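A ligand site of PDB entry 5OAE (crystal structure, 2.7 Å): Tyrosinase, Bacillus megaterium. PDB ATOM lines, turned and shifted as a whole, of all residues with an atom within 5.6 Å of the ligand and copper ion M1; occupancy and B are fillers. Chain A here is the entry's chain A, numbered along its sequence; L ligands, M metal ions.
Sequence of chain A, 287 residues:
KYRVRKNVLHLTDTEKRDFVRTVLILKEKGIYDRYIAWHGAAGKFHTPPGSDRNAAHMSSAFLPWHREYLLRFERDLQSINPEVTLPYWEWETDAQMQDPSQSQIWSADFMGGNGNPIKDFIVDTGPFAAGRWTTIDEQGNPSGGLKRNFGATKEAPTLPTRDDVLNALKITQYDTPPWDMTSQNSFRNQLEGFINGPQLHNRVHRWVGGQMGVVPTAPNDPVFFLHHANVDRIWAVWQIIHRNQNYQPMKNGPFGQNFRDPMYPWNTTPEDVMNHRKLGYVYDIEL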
ATOM      1  N   HIS A  39      -8.713  15.685 -36.065  1.00  0.00           N
ATOM      2  CA  HIS A  39      -8.172  15.038 -34.883  1.00  0.00           C
ATOM      3  C   HIS A  39      -8.569  15.771 -33.613  1.00  0.00           C
ATOM      4  O   HIS A  39      -8.991  15.154 -32.632  1.00  0.00           O
ATOM      5  CB  HIS A  39      -6.644  14.947 -34.983  1.00  0.00           C
ATOM      6  CG  HIS A  39      -6.012  14.181 -33.868  1.00  0.00           C
ATOM      7  ND1 HIS A  39      -5.372  14.790 -32.812  1.00  0.00           N
ATOM      8  CD2 HIS A  39      -5.883  12.850 -33.663  1.00  0.00           C
ATOM      9  CE1 HIS A  39      -4.899  13.867 -31.992  1.00  0.00           C
ATOM     10  NE2 HIS A  39      -5.197  12.683 -32.486  1.00  0.00           N
ATOM     11  N   ALA A  56     -12.076   9.775 -30.594  1.00  0.00           N
ATOM     12  CA  ALA A  56     -10.810   9.298 -31.126  1.00  0.00           C
ATOM     13  C   ALA A  56      -9.887   8.708 -30.072  1.00  0.00           C
ATOM     14  O   ALA A  56      -8.940   7.988 -30.408  1.00  0.00           O
ATOM     15  CB  ALA A  56     -10.103  10.433 -31.851  1.00  0.00           C
ATOM     16  N   HIS A  57     -10.136   9.010 -28.801  1.00  0.00           N
ATOM     17  CA  HIS A  57      -9.211   8.586 -27.751  1.00  0.00           C
ATOM     18  C   HIS A  57      -9.897   8.110 -26.474  1.00  0.00           C
ATOM     19  O   HIS A  57     -11.099   8.306 -26.284  1.00  0.00           O
ATOM     20  CB  HIS A  57      -8.256   9.722 -27.396  1.00  0.00           C
ATOM     21  CG  HIS A  57      -7.571  10.335 -28.589  1.00  0.00           C
ATOM     22  ND1 HIS A  57      -8.064  11.444 -29.236  1.00  0.00           N
ATOM     23  CD2 HIS A  57      -6.445   9.975 -29.245  1.00  0.00           C
ATOM     24  CE1 HIS A  57      -7.261  11.751 -30.239  1.00  0.00           C
ATOM     25  NE2 HIS A  57      -6.272  10.880 -30.273  1.00  0.00           N
ATOM     26  N   PHE A  62     -10.437   4.005 -30.321  1.00  0.00           N
ATOM     27  CA  PHE A  62      -9.130   4.636 -30.501  1.00  0.00           C
ATOM     28  C   PHE A  62      -8.365   4.060 -31.690  1.00  0.00           C
ATOM     29  O   PHE A  62      -7.791   4.803 -32.481  1.00  0.00           O
ATOM     30  CB  PHE A  62      -8.290   4.475 -29.233  1.00  0.00           C
ATOM     31  CG  PHE A  62      -6.820   4.669 -29.451  1.00  0.00           C
ATOM     32  CD1 PHE A  62      -6.294   5.928 -29.685  1.00  0.00           C
ATOM     33  CD2 PHE A  62      -5.946   3.585 -29.413  1.00  0.00           C
ATOM     34  CE1 PHE A  62      -4.930   6.101 -29.891  1.00  0.00           C
ATOM     35  CE2 PHE A  62      -4.597   3.752 -29.613  1.00  0.00           C
ATOM     36  CZ  PHE A  62      -4.085   5.008 -29.851  1.00  0.00           C
ATOM     37  N   TRP A  65     -10.375   4.413 -35.348  1.00  0.00           N
ATOM     38  CA  TRP A  65     -10.441   5.820 -35.732  1.00  0.00           C
ATOM     39  C   TRP A  65      -9.159   6.217 -36.454  1.00  0.00           C
ATOM     40  O   TRP A  65      -9.193   6.758 -37.550  1.00  0.00           O
ATOM     41  CB  TRP A  65     -10.653   6.710 -34.510  1.00  0.00           C
ATOM     42  CG  TRP A  65     -11.020   8.126 -34.837  1.00  0.00           C
ATOM     43  CD1 TRP A  65     -12.285   8.657 -34.870  1.00  0.00           C
ATOM     44  CD2 TRP A  65     -10.127   9.201 -35.162  1.00  0.00           C
ATOM     45  NE1 TRP A  65     -12.223   9.994 -35.208  1.00  0.00           N
ATOM     46  CE2 TRP A  65     -10.922  10.346 -35.389  1.00  0.00           C
ATOM     47  CE3 TRP A  65      -8.742   9.303 -35.295  1.00  0.00           C
ATOM     48  CZ2 TRP A  65     -10.355  11.575 -35.736  1.00  0.00           C
ATOM     49  CZ3 TRP A  65      -8.189  10.527 -35.636  1.00  0.00           C
ATOM     50  CH2 TRP A  65      -9.003  11.641 -35.852  1.00  0.00           C
ATOM     51  N   HIS A  66      -8.028   5.935 -35.817  1.00  0.00           N
ATOM     52  CA  HIS A  66      -6.736   6.323 -36.360  1.00  0.00           C
ATOM     53  C   HIS A  66      -6.370   5.499 -37.594  1.00  0.00           C
ATOM     54  O   HIS A  66      -5.604   5.958 -38.435  1.00  0.00           O
ATOM     55  CB  HIS A  66      -5.656   6.201 -35.290  1.00  0.00           C
ATOM     56  CG  HIS A  66      -5.773   7.233 -34.213  1.00  0.00           C
ATOM     57  ND1 HIS A  66      -6.562   7.054 -33.094  1.00  0.00           N
ATOM     58  CD2 HIS A  66      -5.210   8.465 -34.087  1.00  0.00           C
ATOM     59  CE1 HIS A  66      -6.471   8.129 -32.316  1.00  0.00           C
ATOM     60  NE2 HIS A  66      -5.657   8.993 -32.897  1.00  0.00           N
ATOM     61  N   GLY A 193      -2.024   3.207 -23.907  1.00  0.00           N
ATOM     62  CA  GLY A 193      -0.984   3.508 -22.941  1.00  0.00           C
ATOM     63  C   GLY A 193      -1.455   4.059 -21.614  1.00  0.00           C
ATOM     64  O   GLY A 193      -0.746   4.851 -20.984  1.00  0.00           O
ATOM     65  N   PHE A 194      -2.646   3.667 -21.175  1.00  0.00           N
ATOM     66  CA  PHE A 194      -3.168   4.159 -19.905  1.00  0.00           C
ATOM     67  C   PHE A 194      -2.902   3.175 -18.768  1.00  0.00           C
ATOM     68  O   PHE A 194      -3.117   3.495 -17.601  1.00  0.00           O
ATOM     69  CB  PHE A 194      -4.664   4.466 -20.033  1.00  0.00           C
ATOM     70  CG  PHE A 194      -4.956   5.667 -20.874  1.00  0.00           C
ATOM     71  CD1 PHE A 194      -4.599   6.940 -20.451  1.00  0.00           C
ATOM     72  CD2 PHE A 194      -5.598   5.532 -22.098  1.00  0.00           C
ATOM     73  CE1 PHE A 194      -4.871   8.047 -21.225  1.00  0.00           C
ATOM     74  CE2 PHE A 194      -5.867   6.642 -22.881  1.00  0.00           C
ATOM     75  CZ  PHE A 194      -5.507   7.905 -22.438  1.00  0.00           C
ATOM     76  N   GLY A 197       0.248   4.479 -17.203  1.00  0.00           N
ATOM     77  CA  GLY A 197       0.694   5.401 -18.215  1.00  0.00           C
ATOM     78  C   GLY A 197       1.642   6.473 -17.697  1.00  0.00           C
ATOM     79  O   GLY A 197       1.772   6.657 -16.489  1.00  0.00           O
ATOM     80  N   PRO A 198       2.289   7.176 -18.617  1.00  0.00           N
ATOM     81  CA  PRO A 198       2.113   6.928 -20.050  1.00  0.00           C
ATOM     82  C   PRO A 198       2.980   5.770 -20.536  1.00  0.00           C
ATOM     83  O   PRO A 198       4.125   5.636 -20.105  1.00  0.00           O
ATOM     84  CB  PRO A 198       2.572   8.234 -20.690  1.00  0.00           C
ATOM     85  CG  PRO A 198       3.565   8.797 -19.729  1.00  0.00           C
ATOM     86  CD  PRO A 198       3.065   8.404 -18.358  1.00  0.00           C
ATOM     87  N   GLN A 199       2.463   4.959 -21.430  1.00  0.00           N
ATOM     88  CA  GLN A 199       3.246   3.865 -21.973  1.00  0.00           C
ATOM     89  C   GLN A 199       2.903   3.642 -23.430  1.00  0.00           C
ATOM     90  O   GLN A 199       1.870   4.032 -23.882  1.00  0.00           O
ATOM     91  CB  GLN A 199       3.070   2.607 -21.150  1.00  0.00           C
ATOM     92  CG  GLN A 199       3.252   2.834 -19.668  1.00  0.00           C
ATOM     93  CD  GLN A 199       4.634   2.498 -19.184  1.00  0.00           C
ATOM     94  OE1 GLN A 199       5.452   2.001 -19.932  1.00  0.00           O
ATOM     95  NE2 GLN A 199       4.907   2.781 -17.930  1.00  0.00           N
ATOM     96  N   HIS A 201       2.059   3.931 -27.026  1.00  0.00           N
ATOM     97  CA  HIS A 201       1.533   5.055 -27.804  1.00  0.00           C
ATOM     98  C   HIS A 201       1.543   6.375 -27.032  1.00  0.00           C
ATOM     99  O   HIS A 201       2.028   7.386 -27.542  1.00  0.00           O
ATOM    100  CB  HIS A 201       0.114   4.733 -28.275  1.00  0.00           C
ATOM    101  CG  HIS A 201      -0.672   5.939 -28.696  1.00  0.00           C
ATOM    102  ND1 HIS A 201      -1.600   6.541 -27.877  1.00  0.00           N
ATOM    103  CD2 HIS A 201      -0.681   6.640 -29.846  1.00  0.00           C
ATOM    104  CE1 HIS A 201      -2.144   7.563 -28.502  1.00  0.00           C
ATOM    105  NE2 HIS A 201      -1.604   7.651 -29.701  1.00  0.00           N
ATOM    106  N   ASN A 202       1.012   6.370 -25.812  1.00  0.00           N
ATOM    107  CA  ASN A 202       0.942   7.576 -25.001  1.00  0.00           C
ATOM    108  C   ASN A 202       2.322   8.082 -24.592  1.00  0.00           C
ATOM    109  O   ASN A 202       2.550   9.288 -24.498  1.00  0.00           O
ATOM    110  CB  ASN A 202       0.084   7.342 -23.753  1.00  0.00           C
ATOM    111  CG  ASN A 202      -1.392   7.256 -24.070  1.00  0.00           C
ATOM    112  OD1 ASN A 202      -1.832   7.630 -25.163  1.00  0.00           O
ATOM    113  ND2 ASN A 202      -2.186   6.771 -23.115  1.00  0.00           N
ATOM    114  N   ARG A 203       3.235   7.152 -24.342  1.00  0.00           N
ATOM    115  CA  ARG A 203       4.593   7.496 -23.942  1.00  0.00           C
ATOM    116  C   ARG A 203       5.371   8.144 -25.074  1.00  0.00           C
ATOM    117  O   ARG A 203       6.145   9.071 -24.862  1.00  0.00           O
ATOM    118  CB  ARG A 203       5.336   6.249 -23.446  1.00  0.00           C
ATOM    119  CG  ARG A 203       6.794   6.474 -23.092  1.00  0.00           C
ATOM    120  CD  ARG A 203       7.423   5.225 -22.518  1.00  0.00           C
ATOM    121  NE  ARG A 203       7.011   4.971 -21.137  1.00  0.00           N
ATOM    122  CZ  ARG A 203       7.746   5.257 -20.078  1.00  0.00           C
ATOM    123  NH1 ARG A 203       8.950   5.791 -20.230  1.00  0.00           N
ATOM    124  NH2 ARG A 203       7.291   4.998 -18.855  1.00  0.00           N
ATOM    125  N   HIS A 205       4.167   9.972 -27.496  1.00  0.00           N
ATOM    126  CA  HIS A 205       3.684  11.349 -27.607  1.00  0.00           C
ATOM    127  C   HIS A 205       4.418  12.237 -26.613  1.00  0.00           C
ATOM    128  O   HIS A 205       4.984  13.274 -26.982  1.00  0.00           O
ATOM    129  CB  HIS A 205       2.178  11.424 -27.358  1.00  0.00           C
ATOM    130  CG  HIS A 205       1.342  11.111 -28.563  1.00  0.00           C
ATOM    131  ND1 HIS A 205       1.222  11.981 -29.627  1.00  0.00           N
ATOM    132  CD2 HIS A 205       0.587  10.033 -28.878  1.00  0.00           C
ATOM    133  CE1 HIS A 205       0.437  11.447 -30.543  1.00  0.00           C
ATOM    134  NE2 HIS A 205       0.037  10.267 -30.114  1.00  0.00           N
ATOM    135  N   ARG A 206       4.381  11.849 -25.341  1.00  0.00           N
ATOM    136  CA  ARG A 206       5.020  12.621 -24.280  1.00  0.00           C
ATOM    137  C   ARG A 206       6.529  12.714 -24.437  1.00  0.00           C
ATOM    138  O   ARG A 206       7.139  13.695 -24.031  1.00  0.00           O
ATOM    139  CB  ARG A 206       4.668  12.021 -22.909  1.00  0.00           C
ATOM    140  CG  ARG A 206       3.180  12.018 -22.600  1.00  0.00           C
ATOM    141  CD  ARG A 206       2.859  12.932 -21.420  1.00  0.00           C
ATOM    142  NE  ARG A 206       1.934  12.310 -20.485  1.00  0.00           N
ATOM    143  CZ  ARG A 206       1.780  12.696 -19.225  1.00  0.00           C
ATOM    144  NH1 ARG A 206       2.489  13.705 -18.746  1.00  0.00           N
ATOM    145  NH2 ARG A 206       0.910  12.062 -18.437  1.00  0.00           N
ATOM    146  N   MET A 212       3.396  17.387 -30.066  1.00  0.00           N
ATOM    147  CA  MET A 212       3.092  15.975 -29.897  1.00  0.00           C
ATOM    148  C   MET A 212       2.742  15.641 -28.445  1.00  0.00           C
ATOM    149  O   MET A 212       2.268  14.546 -28.151  1.00  0.00           O
ATOM    150  CB  MET A 212       4.271  15.114 -30.347  1.00  0.00           C
ATOM    151  CG  MET A 212       4.476  15.057 -31.847  1.00  0.00           C
ATOM    152  SD  MET A 212       3.385  13.873 -32.676  1.00  0.00           S
ATOM    153  CE  MET A 212       3.879  12.346 -31.881  1.00  0.00           C
ATOM    154  N   GLY A 213       2.960  16.596 -27.548  1.00  0.00           N
ATOM    155  CA  GLY A 213       2.725  16.356 -26.133  1.00  0.00           C
ATOM    156  C   GLY A 213       1.262  16.471 -25.759  1.00  0.00           C
ATOM    157  O   GLY A 213       0.836  15.914 -24.744  1.00  0.00           O
ATOM    158  N   VAL A 214       0.481  17.175 -26.576  1.00  0.00           N
ATOM    159  CA  VAL A 214      -0.936  17.330 -26.319  1.00  0.00           C
ATOM    160  C   VAL A 214      -1.787  16.852 -27.502  1.00  0.00           C
ATOM    161  O   VAL A 214      -1.327  16.831 -28.639  1.00  0.00           O
ATOM    162  CB  VAL A 214      -1.295  18.808 -25.989  1.00  0.00           C
ATOM    163  CG1 VAL A 214      -0.415  19.326 -24.864  1.00  0.00           C
ATOM    164  CG2 VAL A 214      -1.147  19.668 -27.223  1.00  0.00           C
ATOM    165  N   VAL A 215      -3.023  16.453 -27.211  1.00  0.00           N
ATOM    166  CA  VAL A 215      -3.895  15.868 -28.223  1.00  0.00           C
ATOM    167  C   VAL A 215      -4.291  16.800 -29.391  1.00  0.00           C
ATOM    168  O   VAL A 215      -4.104  16.431 -30.544  1.00  0.00           O
ATOM    169  CB  VAL A 215      -5.194  15.327 -27.569  1.00  0.00           C
ATOM    170  CG1 VAL A 215      -6.134  14.757 -28.624  1.00  0.00           C
ATOM    171  CG2 VAL A 215      -4.851  14.276 -26.524  1.00  0.00           C
ATOM    172  N   ALA A 218      -1.205  17.693 -31.804  1.00  0.00           N
ATOM    173  CA  ALA A 218      -0.285  16.613 -32.154  1.00  0.00           C
ATOM    174  C   ALA A 218      -0.043  16.437 -33.672  1.00  0.00           C
ATOM    175  O   ALA A 218       1.099  16.233 -34.088  1.00  0.00           O
ATOM    176  CB  ALA A 218      -0.764  15.307 -31.550  1.00  0.00           C
ATOM    177  N   PHE A 224       3.673  12.380 -36.383  1.00  0.00           N
ATOM    178  CA  PHE A 224       2.426  11.870 -35.825  1.00  0.00           C
ATOM    179  C   PHE A 224       1.870  10.732 -36.675  1.00  0.00           C
ATOM    180  O   PHE A 224       1.274   9.791 -36.165  1.00  0.00           O
ATOM    181  CB  PHE A 224       1.392  13.007 -35.710  1.00  0.00           C
ATOM    182  CG  PHE A 224       0.054  12.576 -35.177  1.00  0.00           C
ATOM    183  CD1 PHE A 224      -0.191  12.573 -33.816  1.00  0.00           C
ATOM    184  CD2 PHE A 224      -0.964  12.193 -36.041  1.00  0.00           C
ATOM    185  CE1 PHE A 224      -1.422  12.182 -33.323  1.00  0.00           C
ATOM    186  CE2 PHE A 224      -2.194  11.802 -35.548  1.00  0.00           C
ATOM    187  CZ  PHE A 224      -2.429  11.796 -34.195  1.00  0.00           C
ATOM    188  N   HIS A 228       1.602   6.675 -35.576  1.00  0.00           N
ATOM    189  CA  HIS A 228       0.349   5.922 -35.569  1.00  0.00           C
ATOM    190  C   HIS A 228       0.337   4.797 -36.592  1.00  0.00           C
ATOM    191  O   HIS A 228      -0.438   3.850 -36.473  1.00  0.00           O
ATOM    192  CB  HIS A 228      -0.835   6.868 -35.796  1.00  0.00           C
ATOM    193  CG  HIS A 228      -1.283   7.568 -34.556  1.00  0.00           C
ATOM    194  ND1 HIS A 228      -2.231   7.034 -33.702  1.00  0.00           N
ATOM    195  CD2 HIS A 228      -0.906   8.738 -34.004  1.00  0.00           C
ATOM    196  CE1 HIS A 228      -2.415   7.851 -32.689  1.00  0.00           C
ATOM    197  NE2 HIS A 228      -1.623   8.901 -32.855  1.00  0.00           N
HETATM  198  C1  LIG L   1      -1.803  13.023 -28.554  1.00  0.00           C
HETATM  199  C2  LIG L   1      -2.523  12.608 -29.670  1.00  0.00           C
HETATM  200  C3  LIG L   1      -1.777  12.226 -27.422  1.00  0.00           C
HETATM  201  C4  LIG L   1      -3.187  11.414 -29.622  1.00  0.00           C
HETATM  202  C5  LIG L   1      -2.465  11.028 -27.391  1.00  0.00           C
HETATM  203  C6  LIG L   1      -3.181  10.621 -28.504  1.00  0.00           C
HETATM  204  C7  LIG L   1      -1.086  12.654 -26.194  1.00  0.00           C
HETATM  205  C8  LIG L   1      -1.618  12.075 -24.956  1.00  0.00           C
HETATM  206  C9  LIG L   1      -1.482  13.057 -23.810  1.00  0.00           C
HETATM  207  C10 LIG L   1      -0.907  10.786 -24.593  1.00  0.00           C
HETATM  208  C11 LIG L   1      -2.084  12.461 -22.551  1.00  0.00           C
HETATM  209  C12 LIG L   1      -1.511  10.205 -23.341  1.00  0.00           C
HETATM  210  N1  LIG L   1      -1.421  11.197 -22.256  1.00  0.00           N
HETATM  211  C13 LIG L   1      -1.145  10.832 -20.978  1.00  0.00           C
HETATM  212  O1  LIG L   1      -1.610  11.444 -20.036  1.00  0.00           O
HETATM  213  C14 LIG L   1      -0.557   9.468 -20.724  1.00  0.00           C
HETATM  214  F1  LIG L   1      -3.902  11.011 -30.713  1.00  0.00           F
HETATM  215 CU    CU M   1      -5.213  10.740 -32.105  1.00  0.00          CU
HETATM  216 CU    CU M   2      -1.529   9.330 -30.906  1.00  0.00          CU
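NH2 of Arg 206 is in hydrogen-bond range of O1 of the ligand (3.0 Å).
The backbone carbonyl oxygen of Phe 62 sits at hydrogen-bond distance from a ring nitrogen (ND1) of His 66 (2.6 Å).
A ring nitrogen (ND1) of His 39 lies close to the backbone carbonyl oxygen (O) of Val 215 (3.1 Å).
The side-chain amide oxygen (OD1) of Asn 202 is in hydrogen-bond range of a ring nitrogen (ND1) of His 201, at 2.9 Å.
The side-chain amide nitrogen (ND2) of Asn 202 sits close to the backbone carbonyl oxygen (O) of Gly 193, at 3.2 Å.
A ring nitrogen (ND1) of His 205 lies within hydrogen-bond range of the backbone carbonyl oxygen of Met 212, 3.1 Å away.
The backbone carbonyl oxygen (O) of Pro 198 sits at hydrogen-bond distance from the guanidinium group (NE) of Arg 203 (3.1 Å).
Residues that only touch the ligand: Asn 202, His 201, His 205, Pro 198, Val 215, Ala 218, His 228, Phe 224, Gly 213 and Val 214.
Hydrophobic or aromatic side chains within 4 Å of the ligand: His 39, His 57, Pro 198, His 201, His 205, Val 215, Ala 218 and Phe 224.
Within 4 Å of the ligand: His 39, His 57, His 66, Pro 198, His 201, Asn 202, His 205, Arg 206, Gly 213, Val 214, Val 215, Ala 218, Phe 224 and His 228.
The nearest printed residue that does not touch the ligand is Met 212 (4.3 Å).
Residues that only touch copper ion M1: Phe 224.
Of the 23 residues printed, 4 come within 4 Å of copper ion M1.
Along chain A the residues within 4 Å of copper ion M1 span positions 39 to 224.
Copper ion M1 is bound by F1 of the ligand, NE2 of His 66, NE2 of His 39 and NE2 of His 57.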
